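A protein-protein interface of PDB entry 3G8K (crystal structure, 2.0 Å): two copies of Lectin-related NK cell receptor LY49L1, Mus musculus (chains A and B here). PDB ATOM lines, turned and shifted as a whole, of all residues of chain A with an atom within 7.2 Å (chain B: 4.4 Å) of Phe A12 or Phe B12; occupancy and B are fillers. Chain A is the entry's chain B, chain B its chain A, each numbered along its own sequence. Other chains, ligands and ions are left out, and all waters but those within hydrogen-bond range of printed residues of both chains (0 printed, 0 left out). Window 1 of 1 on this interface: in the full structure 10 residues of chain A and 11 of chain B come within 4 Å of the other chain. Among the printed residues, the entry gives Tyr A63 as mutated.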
ATOM      1  N   TYR A  10     -13.655 -34.232   5.529  1.00  0.00           N
ATOM      2  CA  TYR A  10     -14.534 -33.586   6.528  1.00  0.00           C
ATOM      3  C   TYR A  10     -14.111 -32.167   6.763  1.00  0.00           C
ATOM      4  O   TYR A  10     -13.012 -31.803   6.479  1.00  0.00           O
ATOM      5  CB  TYR A  10     -14.525 -34.343   7.856  1.00  0.00           C
ATOM      6  CG  TYR A  10     -13.173 -34.613   8.466  1.00  0.00           C
ATOM      7  CD1 TYR A  10     -12.610 -35.869   8.348  1.00  0.00           C
ATOM      8  CD2 TYR A  10     -12.494 -33.656   9.260  1.00  0.00           C
ATOM      9  CE1 TYR A  10     -11.407 -36.160   8.940  1.00  0.00           C
ATOM     10  CE2 TYR A  10     -11.254 -33.960   9.854  1.00  0.00           C
ATOM     11  CZ  TYR A  10     -10.715 -35.222   9.645  1.00  0.00           C
ATOM     12  OH  TYR A  10      -9.516 -35.630  10.175  1.00  0.00           O
ATOM     13  N   TRP A  11     -14.984 -31.298   7.253  1.00  0.00           N
ATOM     14  CA  TRP A  11     -14.473 -29.957   7.484  1.00  0.00           C
ATOM     15  C   TRP A  11     -15.419 -29.339   8.430  1.00  0.00           C
ATOM     16  O   TRP A  11     -16.477 -29.863   8.651  1.00  0.00           O
ATOM     17  CB  TRP A  11     -14.383 -29.185   6.138  1.00  0.00           C
ATOM     18  CG  TRP A  11     -15.731 -28.937   5.398  1.00  0.00           C
ATOM     19  CD1 TRP A  11     -16.462 -27.795   5.436  1.00  0.00           C
ATOM     20  CD2 TRP A  11     -16.423 -29.830   4.454  1.00  0.00           C
ATOM     21  NE1 TRP A  11     -17.542 -27.898   4.596  1.00  0.00           N
ATOM     22  CE2 TRP A  11     -17.546 -29.134   3.987  1.00  0.00           C
ATOM     23  CE3 TRP A  11     -16.147 -31.107   3.932  1.00  0.00           C
ATOM     24  CZ2 TRP A  11     -18.437 -29.676   3.055  1.00  0.00           C
ATOM     25  CZ3 TRP A  11     -17.023 -31.670   3.048  1.00  0.00           C
ATOM     26  CH2 TRP A  11     -18.166 -30.980   2.621  1.00  0.00           C
ATOM     27  N   PHE A  12     -15.087 -28.187   8.965  1.00  0.00           N
ATOM     28  CA  PHE A  12     -16.104 -27.555   9.777  1.00  0.00           C
ATOM     29  C   PHE A  12     -16.129 -26.093   9.680  1.00  0.00           C
ATOM     30  O   PHE A  12     -15.295 -25.556   9.049  1.00  0.00           O
ATOM     31  CB  PHE A  12     -16.189 -28.134  11.192  1.00  0.00           C
ATOM     32  CG  PHE A  12     -14.956 -28.079  11.968  1.00  0.00           C
ATOM     33  CD1 PHE A  12     -14.588 -26.869  12.624  1.00  0.00           C
ATOM     34  CD2 PHE A  12     -14.230 -29.233  12.176  1.00  0.00           C
ATOM     35  CE1 PHE A  12     -13.386 -26.799  13.438  1.00  0.00           C
ATOM     36  CE2 PHE A  12     -13.062 -29.209  12.951  1.00  0.00           C
ATOM     37  CZ  PHE A  12     -12.628 -27.974  13.604  1.00  0.00           C
ATOM     38  N   CYS A  13     -17.169 -25.477  10.232  1.00  0.00           N
ATOM     39  CA  CYS A  13     -17.355 -24.061  10.189  1.00  0.00           C
ATOM     40  C   CYS A  13     -17.846 -23.507  11.501  1.00  0.00           C
ATOM     41  O   CYS A  13     -18.523 -24.180  12.283  1.00  0.00           O
ATOM     42  CB  CYS A  13     -18.391 -23.701   9.112  1.00  0.00           C
ATOM     43  SG  CYS A  13     -18.074 -24.509   7.459  1.00  0.00           S
ATOM     44  N   TYR A  14     -17.594 -22.215  11.670  1.00  0.00           N
ATOM     45  CA  TYR A  14     -17.985 -21.510  12.869  1.00  0.00           C
ATOM     46  C   TYR A  14     -18.213 -20.063  12.400  1.00  0.00           C
ATOM     47  O   TYR A  14     -17.285 -19.430  11.934  1.00  0.00           O
ATOM     48  CB  TYR A  14     -16.851 -21.591  13.879  1.00  0.00           C
ATOM     49  CG  TYR A  14     -17.082 -20.844  15.180  1.00  0.00           C
ATOM     50  CD1 TYR A  14     -18.212 -21.115  15.975  1.00  0.00           C
ATOM     51  CD2 TYR A  14     -16.163 -19.884  15.617  1.00  0.00           C
ATOM     52  CE1 TYR A  14     -18.444 -20.449  17.155  1.00  0.00           C
ATOM     53  CE2 TYR A  14     -16.384 -19.183  16.816  1.00  0.00           C
ATOM     54  CZ  TYR A  14     -17.528 -19.487  17.580  1.00  0.00           C
ATOM     55  OH  TYR A  14     -17.758 -18.825  18.792  1.00  0.00           O
ATOM     56  N   LYS A  17     -16.413 -18.624   8.994  1.00  0.00           N
ATOM     57  CA  LYS A  17     -15.155 -19.273   8.637  1.00  0.00           C
ATOM     58  C   LYS A  17     -15.284 -20.826   8.661  1.00  0.00           C
ATOM     59  O   LYS A  17     -15.732 -21.393   9.706  1.00  0.00           O
ATOM     60  CB  LYS A  17     -14.031 -18.884   9.637  1.00  0.00           C
ATOM     61  CG  LYS A  17     -12.634 -18.963   9.005  1.00  0.00           C
ATOM     62  CD  LYS A  17     -11.478 -18.676   9.914  1.00  0.00           C
ATOM     63  CE  LYS A  17     -11.362 -17.208  10.254  1.00  0.00           C
ATOM     64  NZ  LYS A  17     -10.352 -17.095  11.336  1.00  0.00           N
ATOM     65  N   CYS A  18     -14.819 -21.488   7.595  1.00  0.00           N
ATOM     66  CA  CYS A  18     -14.625 -22.961   7.601  1.00  0.00           C
ATOM     67  C   CYS A  18     -13.151 -23.414   7.742  1.00  0.00           C
ATOM     68  O   CYS A  18     -12.275 -22.617   7.528  1.00  0.00           O
ATOM     69  CB  CYS A  18     -15.294 -23.556   6.369  1.00  0.00           C
ATOM     70  SG  CYS A  18     -17.080 -23.155   6.314  1.00  0.00           S
ATOM     71  N   TYR A  19     -12.901 -24.729   7.958  1.00  0.00           N
ATOM     72  CA  TYR A  19     -11.634 -25.286   8.392  1.00  0.00           C
ATOM     73  C   TYR A  19     -11.459 -26.605   7.663  1.00  0.00           C
ATOM     74  O   TYR A  19     -12.349 -27.443   7.709  1.00  0.00           O
ATOM     75  CB  TYR A  19     -11.702 -25.577   9.895  1.00  0.00           C
ATOM     76  CG  TYR A  19     -12.010 -24.236  10.706  1.00  0.00           C
ATOM     77  CD1 TYR A  19     -13.301 -23.952  11.148  1.00  0.00           C
ATOM     78  CD2 TYR A  19     -10.999 -23.364  10.982  1.00  0.00           C
ATOM     79  CE1 TYR A  19     -13.598 -22.721  11.878  1.00  0.00           C
ATOM     80  CE2 TYR A  19     -11.255 -22.095  11.717  1.00  0.00           C
ATOM     81  CZ  TYR A  19     -12.548 -21.823  12.111  1.00  0.00           C
ATOM     82  OH  TYR A  19     -12.774 -20.654  12.890  1.00  0.00           O
ATOM     83  N   TYR A  20     -10.321 -26.771   7.046  1.00  0.00           N
ATOM     84  CA  TYR A  20     -10.077 -27.919   6.113  1.00  0.00           C
ATOM     85  C   TYR A  20      -8.754 -28.508   6.593  1.00  0.00           C
ATOM     86  O   TYR A  20      -7.987 -27.812   7.233  1.00  0.00           O
ATOM     87  CB  TYR A  20     -10.055 -27.445   4.635  1.00  0.00           C
ATOM     88  CG  TYR A  20     -11.263 -26.588   4.242  1.00  0.00           C
ATOM     89  CD1 TYR A  20     -11.225 -25.183   4.394  1.00  0.00           C
ATOM     90  CD2 TYR A  20     -12.442 -27.170   3.747  1.00  0.00           C
ATOM     91  CE1 TYR A  20     -12.326 -24.424   4.061  1.00  0.00           C
ATOM     92  CE2 TYR A  20     -13.515 -26.404   3.371  1.00  0.00           C
ATOM     93  CZ  TYR A  20     -13.471 -25.039   3.581  1.00  0.00           C
ATOM     94  OH  TYR A  20     -14.568 -24.292   3.215  1.00  0.00           O
ATOM     95  N   PHE A  21      -8.535 -29.814   6.318  1.00  0.00           N
ATOM     96  CA  PHE A  21      -7.483 -30.605   6.950  1.00  0.00           C
ATOM     97  C   PHE A  21      -6.831 -31.300   5.818  1.00  0.00           C
ATOM     98  O   PHE A  21      -7.505 -31.988   5.045  1.00  0.00           O
ATOM     99  CB  PHE A  21      -8.056 -31.635   8.020  1.00  0.00           C
ATOM    100  CG  PHE A  21      -8.767 -30.951   9.187  1.00  0.00           C
ATOM    101  CD1 PHE A  21     -10.140 -30.676   9.123  1.00  0.00           C
ATOM    102  CD2 PHE A  21      -8.047 -30.494  10.297  1.00  0.00           C
ATOM    103  CE1 PHE A  21     -10.808 -29.969  10.165  1.00  0.00           C
ATOM    104  CE2 PHE A  21      -8.689 -29.810  11.349  1.00  0.00           C
ATOM    105  CZ  PHE A  21     -10.078 -29.534  11.279  1.00  0.00           C
ATOM    106  N   PHE A  53     -13.514 -22.191  20.606  1.00  0.00           N
ATOM    107  CA  PHE A  53     -14.186 -23.103  19.707  1.00  0.00           C
ATOM    108  C   PHE A  53     -13.248 -24.126  19.080  1.00  0.00           C
ATOM    109  O   PHE A  53     -13.527 -25.320  19.173  1.00  0.00           O
ATOM    110  CB  PHE A  53     -14.958 -22.396  18.597  1.00  0.00           C
ATOM    111  CG  PHE A  53     -15.256 -23.340  17.408  1.00  0.00           C
ATOM    112  CD1 PHE A  53     -16.208 -24.376  17.545  1.00  0.00           C
ATOM    113  CD2 PHE A  53     -14.557 -23.230  16.178  1.00  0.00           C
ATOM    114  CE1 PHE A  53     -16.457 -25.312  16.513  1.00  0.00           C
ATOM    115  CE2 PHE A  53     -14.835 -24.172  15.101  1.00  0.00           C
ATOM    116  CZ  PHE A  53     -15.802 -25.215  15.297  1.00  0.00           C
ATOM    117  N   LEU A  54     -12.129 -23.720  18.461  1.00  0.00           N
ATOM    118  CA  LEU A  54     -11.274 -24.724  17.794  1.00  0.00           C
ATOM    119  C   LEU A  54     -10.672 -25.741  18.742  1.00  0.00           C
ATOM    120  O   LEU A  54     -10.544 -26.894  18.408  1.00  0.00           O
ATOM    121  CB  LEU A  54     -10.178 -24.106  16.930  1.00  0.00           C
ATOM    122  CG  LEU A  54     -10.584 -23.344  15.669  1.00  0.00           C
ATOM    123  CD1 LEU A  54      -9.492 -22.241  15.405  1.00  0.00           C
ATOM    124  CD2 LEU A  54     -10.667 -24.433  14.571  1.00  0.00           C
ATOM    125  N   LEU A  56     -12.083 -26.808  21.364  1.00  0.00           N
ATOM    126  CA  LEU A  56     -13.296 -27.676  21.438  1.00  0.00           C
ATOM    127  C   LEU A  56     -13.604 -28.651  20.278  1.00  0.00           C
ATOM    128  O   LEU A  56     -13.856 -29.824  20.541  1.00  0.00           O
ATOM    129  CB  LEU A  56     -14.537 -26.876  21.877  1.00  0.00           C
ATOM    130  CG  LEU A  56     -14.464 -26.545  23.387  1.00  0.00           C
ATOM    131  CD1 LEU A  56     -15.367 -25.365  23.801  1.00  0.00           C
ATOM    132  CD2 LEU A  56     -14.727 -27.799  24.324  1.00  0.00           C
ATOM    133  N   LEU A  57     -13.579 -28.216  19.019  1.00  0.00           N
ATOM    134  CA  LEU A  57     -13.950 -29.112  17.935  1.00  0.00           C
ATOM    135  C   LEU A  57     -12.877 -29.862  17.151  1.00  0.00           C
ATOM    136  O   LEU A  57     -13.231 -30.874  16.521  1.00  0.00           O
ATOM    137  CB  LEU A  57     -15.055 -28.558  16.989  1.00  0.00           C
ATOM    138  CG  LEU A  57     -16.414 -29.367  17.044  1.00  0.00           C
ATOM    139  CD1 LEU A  57     -17.456 -29.234  15.796  1.00  0.00           C
ATOM    140  CD2 LEU A  57     -16.230 -30.902  17.348  1.00  0.00           C
ATOM    141  N   VAL A  58     -11.598 -29.440  17.169  1.00  0.00           N
ATOM    142  CA  VAL A  58     -10.562 -30.135  16.347  1.00  0.00           C
ATOM    143  C   VAL A  58     -10.286 -31.524  16.899  1.00  0.00           C
ATOM    144  O   VAL A  58     -10.168 -31.653  18.121  1.00  0.00           O
ATOM    145  CB  VAL A  58      -9.215 -29.330  16.238  1.00  0.00           C
ATOM    146  CG1 VAL A  58      -9.410 -28.052  15.463  1.00  0.00           C
ATOM    147  CG2 VAL A  58      -8.513 -29.072  17.630  1.00  0.00           C
ATOM    148  N   PRO A  59     -10.193 -32.590  16.038  1.00  0.00           N
ATOM    149  CA  PRO A  59      -9.711 -33.830  16.621  1.00  0.00           C
ATOM    150  C   PRO A  59      -8.460 -33.584  17.439  1.00  0.00           C
ATOM    151  O   PRO A  59      -7.843 -32.516  17.311  1.00  0.00           O
ATOM    152  CB  PRO A  59      -9.410 -34.719  15.390  1.00  0.00           C
ATOM    153  CG  PRO A  59     -10.418 -34.304  14.372  1.00  0.00           C
ATOM    154  CD  PRO A  59     -10.553 -32.752  14.621  1.00  0.00           C
ATOM    155  N   TYR A  63      -1.460 -29.013  15.025  1.00  0.00           N
ATOM    156  CA  TYR A  63      -1.793 -28.456  13.712  1.00  0.00           C
ATOM    157  C   TYR A  63      -0.992 -27.225  13.454  1.00  0.00           C
ATOM    158  O   TYR A  63      -0.997 -26.271  14.273  1.00  0.00           O
ATOM    159  CB  TYR A  63      -3.278 -28.032  13.632  1.00  0.00           C
ATOM    160  CG  TYR A  63      -4.230 -29.129  13.870  1.00  0.00           C
ATOM    161  CD1 TYR A  63      -4.679 -29.929  12.824  1.00  0.00           C
ATOM    162  CD2 TYR A  63      -4.666 -29.418  15.147  1.00  0.00           C
ATOM    163  CE1 TYR A  63      -5.540 -30.955  13.053  1.00  0.00           C
ATOM    164  CE2 TYR A  63      -5.519 -30.445  15.385  1.00  0.00           C
ATOM    165  CZ  TYR A  63      -5.958 -31.222  14.332  1.00  0.00           C
ATOM    166  OH  TYR A  63      -6.863 -32.224  14.604  1.00  0.00           O
ATOM    167  N   ILE A 120      -4.074 -27.028   9.171  1.00  0.00           N
ATOM    168  CA  ILE A 120      -5.442 -26.602   9.284  1.00  0.00           C
ATOM    169  C   ILE A 120      -5.451 -25.274   8.421  1.00  0.00           C
ATOM    170  O   ILE A 120      -4.701 -24.305   8.682  1.00  0.00           O
ATOM    171  CB  ILE A 120      -5.883 -26.524  10.803  1.00  0.00           C
ATOM    172  CG1 ILE A 120      -7.405 -26.472  11.027  1.00  0.00           C
ATOM    173  CG2 ILE A 120      -5.275 -25.291  11.517  1.00  0.00           C
ATOM    174  CD1 ILE A 120      -7.978 -25.396  10.349  1.00  0.00           C
ATOM    175  N   CYS A 121      -6.222 -25.329   7.326  1.00  0.00           N
ATOM    176  CA  CYS A 121      -6.397 -24.240   6.352  1.00  0.00           C
ATOM    177  C   CYS A 121      -7.703 -23.538   6.622  1.00  0.00           C
ATOM    178  O   CYS A 121      -8.703 -24.171   6.757  1.00  0.00           O
ATOM    179  CB  CYS A 121      -6.479 -24.782   4.942  1.00  0.00           C
ATOM    180  SG  CYS A 121      -5.048 -25.777   4.448  1.00  0.00           S
ATOM    181  N   LYS A 123     -10.728 -20.575   5.433  1.00  0.00           N
ATOM    182  CA  LYS A 123     -11.383 -19.860   4.317  1.00  0.00           C
ATOM    183  C   LYS A 123     -12.706 -19.241   4.768  1.00  0.00           C
ATOM    184  O   LYS A 123     -13.579 -19.978   5.179  1.00  0.00           O
ATOM    185  CB  LYS A 123     -11.596 -20.733   3.057  1.00  0.00           C
ATOM    186  CG  LYS A 123     -11.701 -19.823   1.781  1.00  0.00           C
ATOM    187  CD  LYS A 123     -12.199 -20.559   0.561  1.00  0.00           C
ATOM    188  CE  LYS A 123     -12.892 -19.643  -0.478  1.00  0.00           C
ATOM    189  NZ  LYS A 123     -12.055 -19.512  -1.741  1.00  0.00           N
ATOM    190  N   TRP B  11     -20.786 -26.195  12.672  1.00  0.00           N
ATOM    191  CA  TRP B  11     -21.442 -27.322  12.054  1.00  0.00           C
ATOM    192  C   TRP B  11     -20.371 -28.099  11.352  1.00  0.00           C
ATOM    193  O   TRP B  11     -19.285 -27.652  11.258  1.00  0.00           O
ATOM    194  CB  TRP B  11     -22.568 -26.877  11.090  1.00  0.00           C
ATOM    195  CG  TRP B  11     -22.171 -26.082   9.807  1.00  0.00           C
ATOM    196  CD1 TRP B  11     -22.025 -26.582   8.532  1.00  0.00           C
ATOM    197  CD2 TRP B  11     -21.950 -24.651   9.701  1.00  0.00           C
ATOM    198  NE1 TRP B  11     -21.746 -25.559   7.652  1.00  0.00           N
ATOM    199  CE2 TRP B  11     -21.677 -24.371   8.341  1.00  0.00           C
ATOM    200  CE3 TRP B  11     -21.995 -23.582  10.621  1.00  0.00           C
ATOM    201  CZ2 TRP B  11     -21.410 -23.085   7.887  1.00  0.00           C
ATOM    202  CZ3 TRP B  11     -21.733 -22.327  10.181  1.00  0.00           C
ATOM    203  CH2 TRP B  11     -21.452 -22.071   8.832  1.00  0.00           C
ATOM    204  N   PHE B  12     -20.654 -29.298  10.898  1.00  0.00           N
ATOM    205  CA  PHE B  12     -19.598 -29.977  10.151  1.00  0.00           C
ATOM    206  C   PHE B  12     -20.117 -30.840   9.033  1.00  0.00           C
ATOM    207  O   PHE B  12     -21.319 -31.020   8.945  1.00  0.00           O
ATOM    208  CB  PHE B  12     -18.539 -30.597  11.090  1.00  0.00           C
ATOM    209  CG  PHE B  12     -19.054 -31.618  12.031  1.00  0.00           C
ATOM    210  CD1 PHE B  12     -19.311 -32.937  11.578  1.00  0.00           C
ATOM    211  CD2 PHE B  12     -19.161 -31.331  13.379  1.00  0.00           C
ATOM    212  CE1 PHE B  12     -19.787 -33.962  12.484  1.00  0.00           C
ATOM    213  CE2 PHE B  12     -19.599 -32.316  14.289  1.00  0.00           C
ATOM    214  CZ  PHE B  12     -19.923 -33.661  13.843  1.00  0.00           C
ATOM    215  N   CYS B  13     -19.219 -31.240   8.132  1.00  0.00           N
ATOM    216  CA  CYS B  13     -19.606 -31.933   6.944  1.00  0.00           C
ATOM    217  C   CYS B  13     -18.682 -33.099   6.742  1.00  0.00           C
ATOM    218  O   CYS B  13     -17.537 -33.082   7.171  1.00  0.00           O
ATOM    219  CB  CYS B  13     -19.601 -30.991   5.716  1.00  0.00           C
ATOM    220  SG  CYS B  13     -20.645 -29.476   5.930  1.00  0.00           S
ATOM    221  N   LYS B  17     -22.863 -34.735   3.191  1.00  0.00           N
ATOM    222  CA  LYS B  17     -23.810 -34.484   4.286  1.00  0.00           C
ATOM    223  C   LYS B  17     -23.193 -33.496   5.343  1.00  0.00           C
ATOM    224  O   LYS B  17     -22.065 -33.708   5.804  1.00  0.00           O
ATOM    225  CB  LYS B  17     -24.245 -35.810   5.007  1.00  0.00           C
ATOM    226  CG  LYS B  17     -25.477 -35.635   5.978  1.00  0.00           C
ATOM    227  CD  LYS B  17     -26.133 -36.927   6.528  1.00  0.00           C
ATOM    228  CE  LYS B  17     -26.013 -38.134   5.598  1.00  0.00           C
ATOM    229  NZ  LYS B  17     -26.351 -39.298   6.432  1.00  0.00           N
ATOM    230  N   CYS B  18     -23.927 -32.462   5.735  1.00  0.00           N
ATOM    231  CA  CYS B  18     -23.549 -31.646   6.924  1.00  0.00           C
ATOM    232  C   CYS B  18     -24.394 -31.957   8.172  1.00  0.00           C
ATOM    233  O   CYS B  18     -25.372 -32.654   8.044  1.00  0.00           O
ATOM    234  CB  CYS B  18     -23.606 -30.203   6.539  1.00  0.00           C
ATOM    235  SG  CYS B  18     -22.438 -29.903   5.140  1.00  0.00           S
ATOM    236  N   TYR B  19     -24.008 -31.422   9.358  1.00  0.00           N
ATOM    237  CA  TYR B  19     -24.504 -31.799  10.666  1.00  0.00           C
ATOM    238  C   TYR B  19     -24.614 -30.532  11.462  1.00  0.00           C
ATOM    239  O   TYR B  19     -23.635 -29.804  11.615  1.00  0.00           O
ATOM    240  CB  TYR B  19     -23.489 -32.704  11.365  1.00  0.00           C
ATOM    241  CG  TYR B  19     -23.205 -33.983  10.523  1.00  0.00           C
ATOM    242  CD1 TYR B  19     -22.076 -34.050   9.665  1.00  0.00           C
ATOM    243  CD2 TYR B  19     -24.057 -35.070  10.583  1.00  0.00           C
ATOM    244  CE1 TYR B  19     -21.822 -35.236   8.849  1.00  0.00           C
ATOM    245  CE2 TYR B  19     -23.790 -36.273   9.776  1.00  0.00           C
ATOM    246  CZ  TYR B  19     -22.712 -36.276   8.902  1.00  0.00           C
ATOM    247  OH  TYR B  19     -22.402 -37.437   8.197  1.00  0.00           O
ATOM    248  N   PHE B  21     -26.516 -28.492  15.097  1.00  0.00           N
ATOM    249  CA  PHE B  21     -26.725 -28.802  16.513  1.00  0.00           C
ATOM    250  C   PHE B  21     -27.667 -27.763  17.033  1.00  0.00           C
ATOM    251  O   PHE B  21     -27.391 -26.593  16.838  1.00  0.00           O
ATOM    252  CB  PHE B  21     -25.378 -28.815  17.357  1.00  0.00           C
ATOM    253  CG  PHE B  21     -24.372 -29.755  16.806  1.00  0.00           C
ATOM    254  CD1 PHE B  21     -23.595 -29.364  15.714  1.00  0.00           C
ATOM    255  CD2 PHE B  21     -24.270 -31.111  17.283  1.00  0.00           C
ATOM    256  CE1 PHE B  21     -22.706 -30.274  15.086  1.00  0.00           C
ATOM    257  CE2 PHE B  21     -23.331 -32.023  16.683  1.00  0.00           C
ATOM    258  CZ  PHE B  21     -22.566 -31.592  15.576  1.00  0.00           C
ATOM    259  N   PHE B  53     -16.857 -41.753  11.617  1.00  0.00           N
ATOM    260  CA  PHE B  53     -16.596 -40.334  11.612  1.00  0.00           C
ATOM    261  C   PHE B  53     -17.362 -39.531  12.688  1.00  0.00           C
ATOM    262  O   PHE B  53     -16.762 -38.722  13.420  1.00  0.00           O
ATOM    263  CB  PHE B  53     -16.837 -39.732  10.228  1.00  0.00           C
ATOM    264  CG  PHE B  53     -17.186 -38.258  10.300  1.00  0.00           C
ATOM    265  CD1 PHE B  53     -16.169 -37.305  10.552  1.00  0.00           C
ATOM    266  CD2 PHE B  53     -18.525 -37.821  10.165  1.00  0.00           C
ATOM    267  CE1 PHE B  53     -16.467 -35.937  10.675  1.00  0.00           C
ATOM    268  CE2 PHE B  53     -18.840 -36.462  10.308  1.00  0.00           C
ATOM    269  CZ  PHE B  53     -17.803 -35.501  10.544  1.00  0.00           C
ATOM    270  N   LEU B  54     -18.671 -39.731  12.828  1.00  0.00           N
ATOM    271  CA  LEU B  54     -19.375 -38.907  13.808  1.00  0.00           C
ATOM    272  C   LEU B  54     -18.855 -39.147  15.204  1.00  0.00           C
ATOM    273  O   LEU B  54     -18.736 -38.215  15.964  1.00  0.00           O
ATOM    274  CB  LEU B  54     -20.894 -39.065  13.751  1.00  0.00           C
ATOM    275  CG  LEU B  54     -21.585 -38.338  12.598  1.00  0.00           C
ATOM    276  CD1 LEU B  54     -22.852 -39.165  12.220  1.00  0.00           C
ATOM    277  CD2 LEU B  54     -21.887 -36.912  13.035  1.00  0.00           C
ATOM    278  N   LEU B  57     -15.680 -37.105  15.403  1.00  0.00           N
ATOM    279  CA  LEU B  57     -15.865 -35.666  15.349  1.00  0.00           C
ATOM    280  C   LEU B  57     -16.839 -34.961  16.264  1.00  0.00           C
ATOM    281  O   LEU B  57     -16.643 -33.778  16.490  1.00  0.00           O
ATOM    282  CB  LEU B  57     -16.213 -35.253  13.932  1.00  0.00           C
ATOM    283  CG  LEU B  57     -15.147 -34.430  13.207  1.00  0.00           C
ATOM    284  CD1 LEU B  57     -14.458 -33.359  14.174  1.00  0.00           C
ATOM    285  CD2 LEU B  57     -14.077 -35.337  12.520  1.00  0.00           C
ATOM    286  N   VAL B  58     -17.916 -35.603  16.744  1.00  0.00           N
ATOM    287  CA  VAL B  58     -18.900 -34.881  17.604  1.00  0.00           C
ATOM    288  C   VAL B  58     -18.283 -34.495  18.959  1.00  0.00           C
ATOM    289  O   VAL B  58     -17.530 -35.295  19.492  1.00  0.00           O
ATOM    290  CB  VAL B  58     -20.197 -35.708  17.834  1.00  0.00           C
ATOM    291  CG1 VAL B  58     -21.000 -35.781  16.604  1.00  0.00           C
ATOM    292  CG2 VAL B  58     -19.925 -37.137  18.420  1.00  0.00           C
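Trp A11 touches Phe B12, and with the chains exchanged Phe A12 touches Trp B11.
Trp A11 touches Cys B13, and with the chains exchanged Cys A13 touches Trp B11.
Phe A12 touches its own counterpart, Phe B12.
Leu A57 touches Phe B12, but with the chains exchanged Phe A12 does not touch Leu B57 (4.5 Å).
Positions printed for both chains: 11, 12, 13, 17, 18, 19, 21, 53, 54, 57 and 58.
The backbone carbonyl oxygen (O) of Phe B12 is in hydrogen-bond range of the backbone NH (N) of Tyr B19 (2.8 Å).
SG of Cys B13 forms a disulfide with SG of Cys B18.
The backbone NH (N) of Tyr A19 lies within hydrogen-bond range of the backbone carbonyl oxygen (O) of Phe A12 (2.8 Å).
SG of Cys A13 forms a disulfide with SG of Cys A18, 2.0 Å away.
The backbone carbonyl oxygen (O) of Pro A59 sits at hydrogen-bond distance from the side-chain hydroxyl (OH) of Tyr A63, at 2.9 Å.
Phe A12 touches just these residues of chain B: Trp B11 and Phe B12.
Phe B12 touches three residues of chain A.
Printed residues of chain B within 4 Å of Trp A11: Phe B12 and Cys B13.
Printed residues of chain A within 4 Å of Trp B11: Phe A12 and Cys A13.
Of the printed residues of chain A, Cys B13 touches Tyr A10 and Trp A11.
Phe B21 touches none of the printed residues of chain A.
The nearest printed residue of chain B that does not touch Phe A12 is Leu B57 (4.5 Å).
N of Trp B11 is in hydrogen-bond range of O of Cys A13, 3.1 Å away.
The backbone NH (N) of Cys B13 sits at hydrogen-bond distance from the backbone carbonyl oxygen (O) of Trp A11 (3.1 Å).
Among the printed residues, merely in contact across the chains: Leu A57 with Leu B57, Tyr A10 with Cys B13, Phe A12 with Trp B11, Trp A11 with Phe B12, Phe A12 with Phe B12, Leu A57 with Phe B12, Tyr A10 with Phe B53, Pro A59 with Leu B57 and Tyr A10 with Leu B57.
Printed residues of chain A that touch a printed residue of chain B: Tyr A10, Trp A11, Phe A12, Cys A13, Leu A57 and Pro A59.
Along chain A the printed residues that touch a printed residue of chain B span positions 10 to 59.
Printed residues of chain B that touch a printed residue of chain A: Trp B11, Phe B12, Cys B13, Phe B53 and Leu B57.
Hydrophobic or aromatic side chains of chain B within 4 Å of the printed part of chain A: Trp B11, Phe B12, Phe B53 and Leu B57.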
